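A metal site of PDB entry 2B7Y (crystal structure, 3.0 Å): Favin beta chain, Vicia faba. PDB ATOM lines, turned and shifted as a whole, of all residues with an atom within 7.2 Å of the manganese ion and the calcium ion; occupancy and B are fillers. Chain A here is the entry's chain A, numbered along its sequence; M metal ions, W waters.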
ATOM      1  N   ASP A  82      15.015   9.217  15.270  1.00  0.00           N
ATOM      2  CA  ASP A  82      15.328   9.268  16.679  1.00  0.00           C
ATOM      3  C   ASP A  82      14.740   7.990  17.264  1.00  0.00           C
ATOM      4  O   ASP A  82      15.214   7.456  18.285  1.00  0.00           O
ATOM      5  CB  ASP A  82      14.584  10.467  17.249  1.00  0.00           C
ATOM      6  CG  ASP A  82      15.483  11.428  17.965  1.00  0.00           C
ATOM      7  OD1 ASP A  82      15.882  12.460  17.352  1.00  0.00           O
ATOM      8  OD2 ASP A  82      15.834  11.219  19.129  1.00  0.00           O
ATOM      9  N   GLY A  83      13.677   7.523  16.576  1.00  0.00           N
ATOM     10  CA  GLY A  83      13.065   6.224  16.815  1.00  0.00           C
ATOM     11  C   GLY A  83      11.575   6.065  16.535  1.00  0.00           C
ATOM     12  O   GLY A  83      10.888   6.975  16.036  1.00  0.00           O
ATOM     13  N   GLY A  99      11.647  14.907  18.860  1.00  0.00           N
ATOM     14  CA  GLY A  99      12.998  14.298  18.875  1.00  0.00           C
ATOM     15  C   GLY A  99      13.134  13.112  19.802  1.00  0.00           C
ATOM     16  O   GLY A  99      12.346  12.156  19.770  1.00  0.00           O
ATOM     17  N   GLY A 100      14.144  13.182  20.658  1.00  0.00           N
ATOM     18  CA  GLY A 100      14.318  12.192  21.720  1.00  0.00           C
ATOM     19  C   GLY A 100      13.073  11.721  22.466  1.00  0.00           C
ATOM     20  O   GLY A 100      13.060  10.601  22.952  1.00  0.00           O
ATOM     21  N   TYR A 101      12.031  12.531  22.581  1.00  0.00           N
ATOM     22  CA  TYR A 101      10.891  12.044  23.363  1.00  0.00           C
ATOM     23  C   TYR A 101       9.856  11.222  22.526  1.00  0.00           C
ATOM     24  O   TYR A 101       8.825  10.735  23.068  1.00  0.00           O
ATOM     25  CB  TYR A 101      10.254  13.186  24.159  1.00  0.00           C
ATOM     26  CG  TYR A 101      11.236  13.920  25.078  1.00  0.00           C
ATOM     27  CD1 TYR A 101      11.357  13.559  26.446  1.00  0.00           C
ATOM     28  CD2 TYR A 101      12.041  14.964  24.589  1.00  0.00           C
ATOM     29  CE1 TYR A 101      12.256  14.235  27.301  1.00  0.00           C
ATOM     30  CE2 TYR A 101      12.924  15.629  25.416  1.00  0.00           C
ATOM     31  CZ  TYR A 101      13.044  15.272  26.776  1.00  0.00           C
ATOM     32  OH  TYR A 101      13.968  15.949  27.569  1.00  0.00           O
ATOM     33  N   LEU A 102      10.146  11.079  21.211  1.00  0.00           N
ATOM     34  CA  LEU A 102       9.368  10.296  20.259  1.00  0.00           C
ATOM     35  C   LEU A 102       7.865  10.647  20.180  1.00  0.00           C
ATOM     36  O   LEU A 102       7.018   9.817  19.865  1.00  0.00           O
ATOM     37  CB  LEU A 102       9.588   8.809  20.549  1.00  0.00           C
ATOM     38  CG  LEU A 102      11.063   8.468  20.854  1.00  0.00           C
ATOM     39  CD1 LEU A 102      11.184   7.158  21.571  1.00  0.00           C
ATOM     40  CD2 LEU A 102      11.906   8.418  19.615  1.00  0.00           C
ATOM     41  N   GLU A 120       9.690   1.138  22.870  1.00  0.00           N
ATOM     42  CA  GLU A 120      10.480   2.051  22.070  1.00  0.00           C
ATOM     43  C   GLU A 120      11.624   1.372  21.394  1.00  0.00           C
ATOM     44  O   GLU A 120      12.393   0.619  22.033  1.00  0.00           O
ATOM     45  CB  GLU A 120      11.020   3.218  22.917  1.00  0.00           C
ATOM     46  CG  GLU A 120      12.080   2.854  23.953  1.00  0.00           C
ATOM     47  CD  GLU A 120      12.930   4.047  24.383  1.00  0.00           C
ATOM     48  OE1 GLU A 120      13.595   3.997  25.467  1.00  0.00           O
ATOM     49  OE2 GLU A 120      12.939   5.056  23.635  1.00  0.00           O
ATOM     50  N   PHE A 121      11.754   1.639  20.101  1.00  0.00           N
ATOM     51  CA  PHE A 121      12.855   1.097  19.314  1.00  0.00           C
ATOM     52  C   PHE A 121      13.743   2.280  19.026  1.00  0.00           C
ATOM     53  O   PHE A 121      13.585   2.975  18.035  1.00  0.00           O
ATOM     54  CB  PHE A 121      12.332   0.399  18.051  1.00  0.00           C
ATOM     55  CG  PHE A 121      11.333  -0.693  18.352  1.00  0.00           C
ATOM     56  CD1 PHE A 121      10.031  -0.384  18.760  1.00  0.00           C
ATOM     57  CD2 PHE A 121      11.717  -2.054  18.284  1.00  0.00           C
ATOM     58  CE1 PHE A 121       9.117  -1.411  19.081  1.00  0.00           C
ATOM     59  CE2 PHE A 121      10.802  -3.076  18.597  1.00  0.00           C
ATOM     60  CZ  PHE A 121       9.483  -2.743  18.999  1.00  0.00           C
ATOM     61  N   ASP A 122      14.662   2.510  19.937  1.00  0.00           N
ATOM     62  CA  ASP A 122      15.383   3.761  20.001  1.00  0.00           C
ATOM     63  C   ASP A 122      16.595   3.729  19.112  1.00  0.00           C
ATOM     64  O   ASP A 122      17.412   2.812  19.244  1.00  0.00           O
ATOM     65  CB  ASP A 122      15.824   4.013  21.453  1.00  0.00           C
ATOM     66  CG  ASP A 122      16.268   5.428  21.694  1.00  0.00           C
ATOM     67  OD1 ASP A 122      17.224   5.876  21.028  1.00  0.00           O
ATOM     68  OD2 ASP A 122      15.721   6.167  22.552  1.00  0.00           O
ATOM     69  N   THR A 123      16.745   4.705  18.242  1.00  0.00           N
ATOM     70  CA  THR A 123      17.909   4.654  17.358  1.00  0.00           C
ATOM     71  C   THR A 123      18.891   5.819  17.490  1.00  0.00           C
ATOM     72  O   THR A 123      19.777   5.968  16.639  1.00  0.00           O
ATOM     73  CB  THR A 123      17.504   4.499  15.893  1.00  0.00           C
ATOM     74  OG1 THR A 123      16.819   5.681  15.438  1.00  0.00           O
ATOM     75  CG2 THR A 123      16.481   3.406  15.765  1.00  0.00           C
ATOM     76  N   PHE A 124      18.725   6.641  18.536  1.00  0.00           N
ATOM     77  CA  PHE A 124      19.638   7.770  18.760  1.00  0.00           C
ATOM     78  C   PHE A 124      19.961   7.994  20.232  1.00  0.00           C
ATOM     79  O   PHE A 124      19.067   8.203  21.053  1.00  0.00           O
ATOM     80  CB  PHE A 124      19.111   9.059  18.116  1.00  0.00           C
ATOM     81  CG  PHE A 124      20.052  10.258  18.251  1.00  0.00           C
ATOM     82  CD1 PHE A 124      20.117  11.004  19.446  1.00  0.00           C
ATOM     83  CD2 PHE A 124      20.854  10.679  17.167  1.00  0.00           C
ATOM     84  CE1 PHE A 124      20.950  12.109  19.557  1.00  0.00           C
ATOM     85  CE2 PHE A 124      21.719  11.784  17.274  1.00  0.00           C
ATOM     86  CZ  PHE A 124      21.749  12.505  18.470  1.00  0.00           C
ATOM     87  N   TYR A 125      21.262   7.970  20.524  1.00  0.00           N
ATOM     88  CA  TYR A 125      21.781   8.154  21.874  1.00  0.00           C
ATOM     89  C   TYR A 125      21.527   9.569  22.440  1.00  0.00           C
ATOM     90  O   TYR A 125      22.037  10.583  21.980  1.00  0.00           O
ATOM     91  CB  TYR A 125      23.280   7.779  21.950  1.00  0.00           C
ATOM     92  CG  TYR A 125      23.887   7.977  23.322  1.00  0.00           C
ATOM     93  CD1 TYR A 125      23.217   7.488  24.441  1.00  0.00           C
ATOM     94  CD2 TYR A 125      25.115   8.635  23.503  1.00  0.00           C
ATOM     95  CE1 TYR A 125      23.731   7.636  25.696  1.00  0.00           C
ATOM     96  CE2 TYR A 125      25.644   8.799  24.778  1.00  0.00           C
ATOM     97  CZ  TYR A 125      24.934   8.275  25.856  1.00  0.00           C
ATOM     98  OH  TYR A 125      25.341   8.392  27.140  1.00  0.00           O
ATOM     99  N   ASN A 126      20.706   9.630  23.455  1.00  0.00           N
ATOM    100  CA  ASN A 126      20.548  10.873  24.114  1.00  0.00           C
ATOM    101  C   ASN A 126      21.306  10.774  25.442  1.00  0.00           C
ATOM    102  O   ASN A 126      20.855  10.133  26.412  1.00  0.00           O
ATOM    103  CB  ASN A 126      19.072  11.154  24.261  1.00  0.00           C
ATOM    104  CG  ASN A 126      18.355  11.224  22.921  1.00  0.00           C
ATOM    105  OD1 ASN A 126      17.591  10.325  22.599  1.00  0.00           O
ATOM    106  ND2 ASN A 126      18.601  12.284  22.140  1.00  0.00           N
ATOM    107  N   ALA A 127      22.506  11.386  25.440  1.00  0.00           N
ATOM    108  CA  ALA A 127      23.495  11.194  26.501  1.00  0.00           C
ATOM    109  C   ALA A 127      22.812  11.358  27.817  1.00  0.00           C
ATOM    110  O   ALA A 127      23.136  10.705  28.792  1.00  0.00           O
ATOM    111  CB  ALA A 127      24.644  12.197  26.363  1.00  0.00           C
ATOM    112  N   TRP A 129      19.675  10.555  28.832  1.00  0.00           N
ATOM    113  CA  TRP A 129      18.849   9.478  29.469  1.00  0.00           C
ATOM    114  C   TRP A 129      18.946   8.043  29.005  1.00  0.00           C
ATOM    115  O   TRP A 129      18.570   7.150  29.754  1.00  0.00           O
ATOM    116  CB  TRP A 129      17.408   9.833  29.397  1.00  0.00           C
ATOM    117  CG  TRP A 129      16.974   9.967  28.063  1.00  0.00           C
ATOM    118  CD1 TRP A 129      16.627   8.964  27.216  1.00  0.00           C
ATOM    119  CD2 TRP A 129      16.796  11.177  27.372  1.00  0.00           C
ATOM    120  NE1 TRP A 129      16.249   9.493  26.011  1.00  0.00           N
ATOM    121  CE2 TRP A 129      16.333  10.857  26.083  1.00  0.00           C
ATOM    122  CE3 TRP A 129      16.963  12.517  27.718  1.00  0.00           C
ATOM    123  CZ2 TRP A 129      16.048  11.841  25.139  1.00  0.00           C
ATOM    124  CZ3 TRP A 129      16.691  13.491  26.778  1.00  0.00           C
ATOM    125  CH2 TRP A 129      16.234  13.152  25.499  1.00  0.00           C
ATOM    126  N   ASP A 130      19.349   7.854  27.755  1.00  0.00           N
ATOM    127  CA  ASP A 130      19.436   6.516  27.163  1.00  0.00           C
ATOM    128  C   ASP A 130      20.553   5.704  27.853  1.00  0.00           C
ATOM    129  O   ASP A 130      21.334   6.300  28.623  1.00  0.00           O
ATOM    130  CB  ASP A 130      19.672   6.645  25.648  1.00  0.00           C
ATOM    131  CG  ASP A 130      18.389   7.039  24.863  1.00  0.00           C
ATOM    132  OD1 ASP A 130      17.253   6.601  25.210  1.00  0.00           O
ATOM    133  OD2 ASP A 130      18.445   7.792  23.871  1.00  0.00           O
ATOM    134  N   PRO A 131      20.643   4.381  27.643  1.00  0.00           N
ATOM    135  CA  PRO A 131      21.673   3.630  28.276  1.00  0.00           C
ATOM    136  C   PRO A 131      22.959   4.109  27.685  1.00  0.00           C
ATOM    137  O   PRO A 131      22.996   4.631  26.545  1.00  0.00           O
ATOM    138  CB  PRO A 131      21.391   2.197  27.847  1.00  0.00           C
ATOM    139  CG  PRO A 131      20.018   2.180  27.561  1.00  0.00           C
ATOM    140  CD  PRO A 131      19.813   3.497  26.812  1.00  0.00           C
ATOM    141  N   LYS A 135      24.672   2.321  22.683  1.00  0.00           N
ATOM    142  CA  LYS A 135      24.218   1.410  21.633  1.00  0.00           C
ATOM    143  C   LYS A 135      22.721   1.624  21.428  1.00  0.00           C
ATOM    144  O   LYS A 135      22.004   1.876  22.399  1.00  0.00           O
ATOM    145  CB  LYS A 135      24.447  -0.030  22.060  1.00  0.00           C
ATOM    146  CG  LYS A 135      25.883  -0.512  21.967  1.00  0.00           C
ATOM    147  CD  LYS A 135      25.949  -1.960  21.379  1.00  0.00           C
ATOM    148  CE  LYS A 135      27.400  -2.435  21.192  1.00  0.00           C
ATOM    149  NZ  LYS A 135      28.134  -2.414  22.517  1.00  0.00           N
ATOM    150  N   HIS A 137      18.870   0.493  21.024  1.00  0.00           N
ATOM    151  CA  HIS A 137      18.204  -0.336  21.981  1.00  0.00           C
ATOM    152  C   HIS A 137      16.680  -0.297  21.834  1.00  0.00           C
ATOM    153  O   HIS A 137      16.094   0.609  21.225  1.00  0.00           O
ATOM    154  CB  HIS A 137      18.568   0.159  23.372  1.00  0.00           C
ATOM    155  CG  HIS A 137      18.264   1.611  23.585  1.00  0.00           C
ATOM    156  ND1 HIS A 137      19.090   2.617  23.106  1.00  0.00           N
ATOM    157  CD2 HIS A 137      17.227   2.222  24.193  1.00  0.00           C
ATOM    158  CE1 HIS A 137      18.579   3.783  23.434  1.00  0.00           C
ATOM    159  NE2 HIS A 137      17.451   3.572  24.095  1.00  0.00           N
ATOM    160  N   ILE A 138      16.035  -1.300  22.414  1.00  0.00           N
ATOM    161  CA  ILE A 138      14.598  -1.260  22.544  1.00  0.00           C
ATOM    162  C   ILE A 138      14.246  -1.124  24.042  1.00  0.00           C
ATOM    163  O   ILE A 138      15.001  -1.557  24.939  1.00  0.00           O
ATOM    164  CB  ILE A 138      13.968  -2.480  21.878  1.00  0.00           C
ATOM    165  CG1 ILE A 138      13.938  -3.665  22.778  1.00  0.00           C
ATOM    166  CG2 ILE A 138      14.746  -2.959  20.644  1.00  0.00           C
ATOM    167  CD1 ILE A 138      13.751  -4.867  21.949  1.00  0.00           C
ATOM    168  N   GLY A 139      13.144  -0.471  24.337  1.00  0.00           N
ATOM    169  CA  GLY A 139      12.892  -0.189  25.725  1.00  0.00           C
ATOM    170  C   GLY A 139      11.442  -0.154  26.094  1.00  0.00           C
ATOM    171  O   GLY A 139      10.594   0.252  25.300  1.00  0.00           O
ATOM    172  N   ASP A 141       8.957   1.857  28.268  1.00  0.00           N
ATOM    173  CA  ASP A 141       8.927   3.174  28.862  1.00  0.00           C
ATOM    174  C   ASP A 141       7.594   3.294  29.475  1.00  0.00           C
ATOM    175  O   ASP A 141       6.595   2.831  28.902  1.00  0.00           O
ATOM    176  CB  ASP A 141       9.016   4.265  27.798  1.00  0.00           C
ATOM    177  CG  ASP A 141      10.255   4.128  26.946  1.00  0.00           C
ATOM    178  OD1 ASP A 141      11.079   3.200  27.189  1.00  0.00           O
ATOM    179  OD2 ASP A 141      10.508   4.874  25.984  1.00  0.00           O
ATOM    180  N   ILE A 145      10.655   8.939  29.323  1.00  0.00           N
ATOM    181  CA  ILE A 145      11.336   8.614  28.094  1.00  0.00           C
ATOM    182  C   ILE A 145      12.585   7.846  28.473  1.00  0.00           C
ATOM    183  O   ILE A 145      13.410   7.516  27.630  1.00  0.00           O
ATOM    184  CB  ILE A 145      11.706   9.880  27.384  1.00  0.00           C
ATOM    185  CG1 ILE A 145      12.084   9.606  25.937  1.00  0.00           C
ATOM    186  CG2 ILE A 145      12.879  10.536  28.108  1.00  0.00           C
ATOM    187  CD1 ILE A 145      11.179   8.736  25.232  1.00  0.00           C
ATOM    188  N   LYS A 146      12.716   7.576  29.767  1.00  0.00           N
ATOM    189  CA  LYS A 146      13.856   6.856  30.335  1.00  0.00           C
ATOM    190  C   LYS A 146      13.382   5.411  30.689  1.00  0.00           C
ATOM    191  O   LYS A 146      12.659   5.208  31.677  1.00  0.00           O
ATOM    192  CB  LYS A 146      14.307   7.626  31.570  1.00  0.00           C
ATOM    193  CG  LYS A 146      15.689   7.364  32.009  1.00  0.00           C
ATOM    194  CD  LYS A 146      15.717   7.225  33.521  1.00  0.00           C
ATOM    195  CE  LYS A 146      17.133   7.333  34.040  1.00  0.00           C
ATOM    196  NZ  LYS A 146      17.079   7.343  35.516  1.00  0.00           N
ATOM    197  N   SER A 147      13.737   4.430  29.853  1.00  0.00           N
ATOM    198  CA  SER A 147      12.991   3.149  29.821  1.00  0.00           C
ATOM    199  C   SER A 147      13.241   2.394  31.110  1.00  0.00           C
ATOM    200  O   SER A 147      14.364   2.398  31.622  1.00  0.00           O
ATOM    201  CB  SER A 147      13.398   2.279  28.631  1.00  0.00           C
ATOM    202  OG  SER A 147      13.965   3.045  27.572  1.00  0.00           O
ATOM    203  N   THR A 150      15.921  -2.019  28.971  1.00  0.00           N
ATOM    204  CA  THR A 150      16.308  -2.075  27.557  1.00  0.00           C
ATOM    205  C   THR A 150      17.152  -3.310  27.215  1.00  0.00           C
ATOM    206  O   THR A 150      17.789  -3.906  28.093  1.00  0.00           O
ATOM    207  CB  THR A 150      17.171  -0.902  27.218  1.00  0.00           C
ATOM    208  OG1 THR A 150      18.509  -1.386  27.027  1.00  0.00           O
ATOM    209  CG2 THR A 150      17.282   0.082  28.418  1.00  0.00           C
HETATM  210 MN    MN M   1      16.023   5.075  24.718  1.00  0.00          MN
HETATM  211 CA    CA M   2      17.105   7.983  22.278  1.00  0.00          CA
HETATM  212  O   HOH W   1      15.002   8.933  23.380  1.00  0.00           O
HETATM  213  O   HOH W   2      16.321   8.906  20.253  1.00  0.00           O
HETATM  214  O   HOH W   3      16.270   4.778  27.275  1.00  0.00           O
HETATM  215  O   HOH W   4      13.995   6.988  25.537  1.00  0.00           O
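The calcium ion is bound by the side-chain carboxylate (OD2) of Asp 130 (2.1 Å).
The calcium ion is bound by the side-chain carboxylate (OD2) of Asp 122, at 2.3 Å.
The calcium ion is bound by the backbone carbonyl oxygen (O) of Phe 124.
Water W2 is bound to the calcium ion (2.4 Å).
The calcium ion is bound by OD1 of Asn 126, at 2.4 Å.
OD1 of Asp 122 binds the calcium ion, at 2.5 Å.
The calcium ion is bound by water W1 (2.6 Å).
Within 4 Å of the calcium ion: Asp 122, Phe 124, Asn 126 and Asp 130.
Water W3 bridges the side-chain hydroxyl (OG) of Ser 147 (2.9 Å) and the side-chain carboxylate (OE1) of Glu 120 (3.3 Å).
Water W4 lies within hydrogen-bond range of OE2 of Glu 120 (2.9 Å) and NE1 of Trp 129 (3.4 Å).
Water W1 bridges the backbone carbonyl oxygen of Gly 100 (2.6 Å) and the indole nitrogen of Trp 129 (3.0 Å).
A ring nitrogen (ND1) of His 137 is in hydrogen-bond range of the backbone carbonyl oxygen of Lys 135 (3.1 Å).
O of Glu 120 sits at hydrogen-bond distance from N of Gly 139, at 2.7 Å.
OD1 of Asp 130 lies close to NE1 of Trp 129 (3.2 Å).
Along chain A the residues within 4 Å of the manganese ion span positions 120 to 137.
The manganese ion is bound by OD1 of Asp 130 (2.0 Å), NE2 of His 137 (2.2 Å), OD2 of Asp 122 (2.4 Å) and water W3 (2.6 Å).
Slightly farther from the manganese ion lies the side-chain carboxylate (OE1) of Glu 120 (2.8 Å).
Slightly farther from the manganese ion lies water W4 (2.9 Å).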
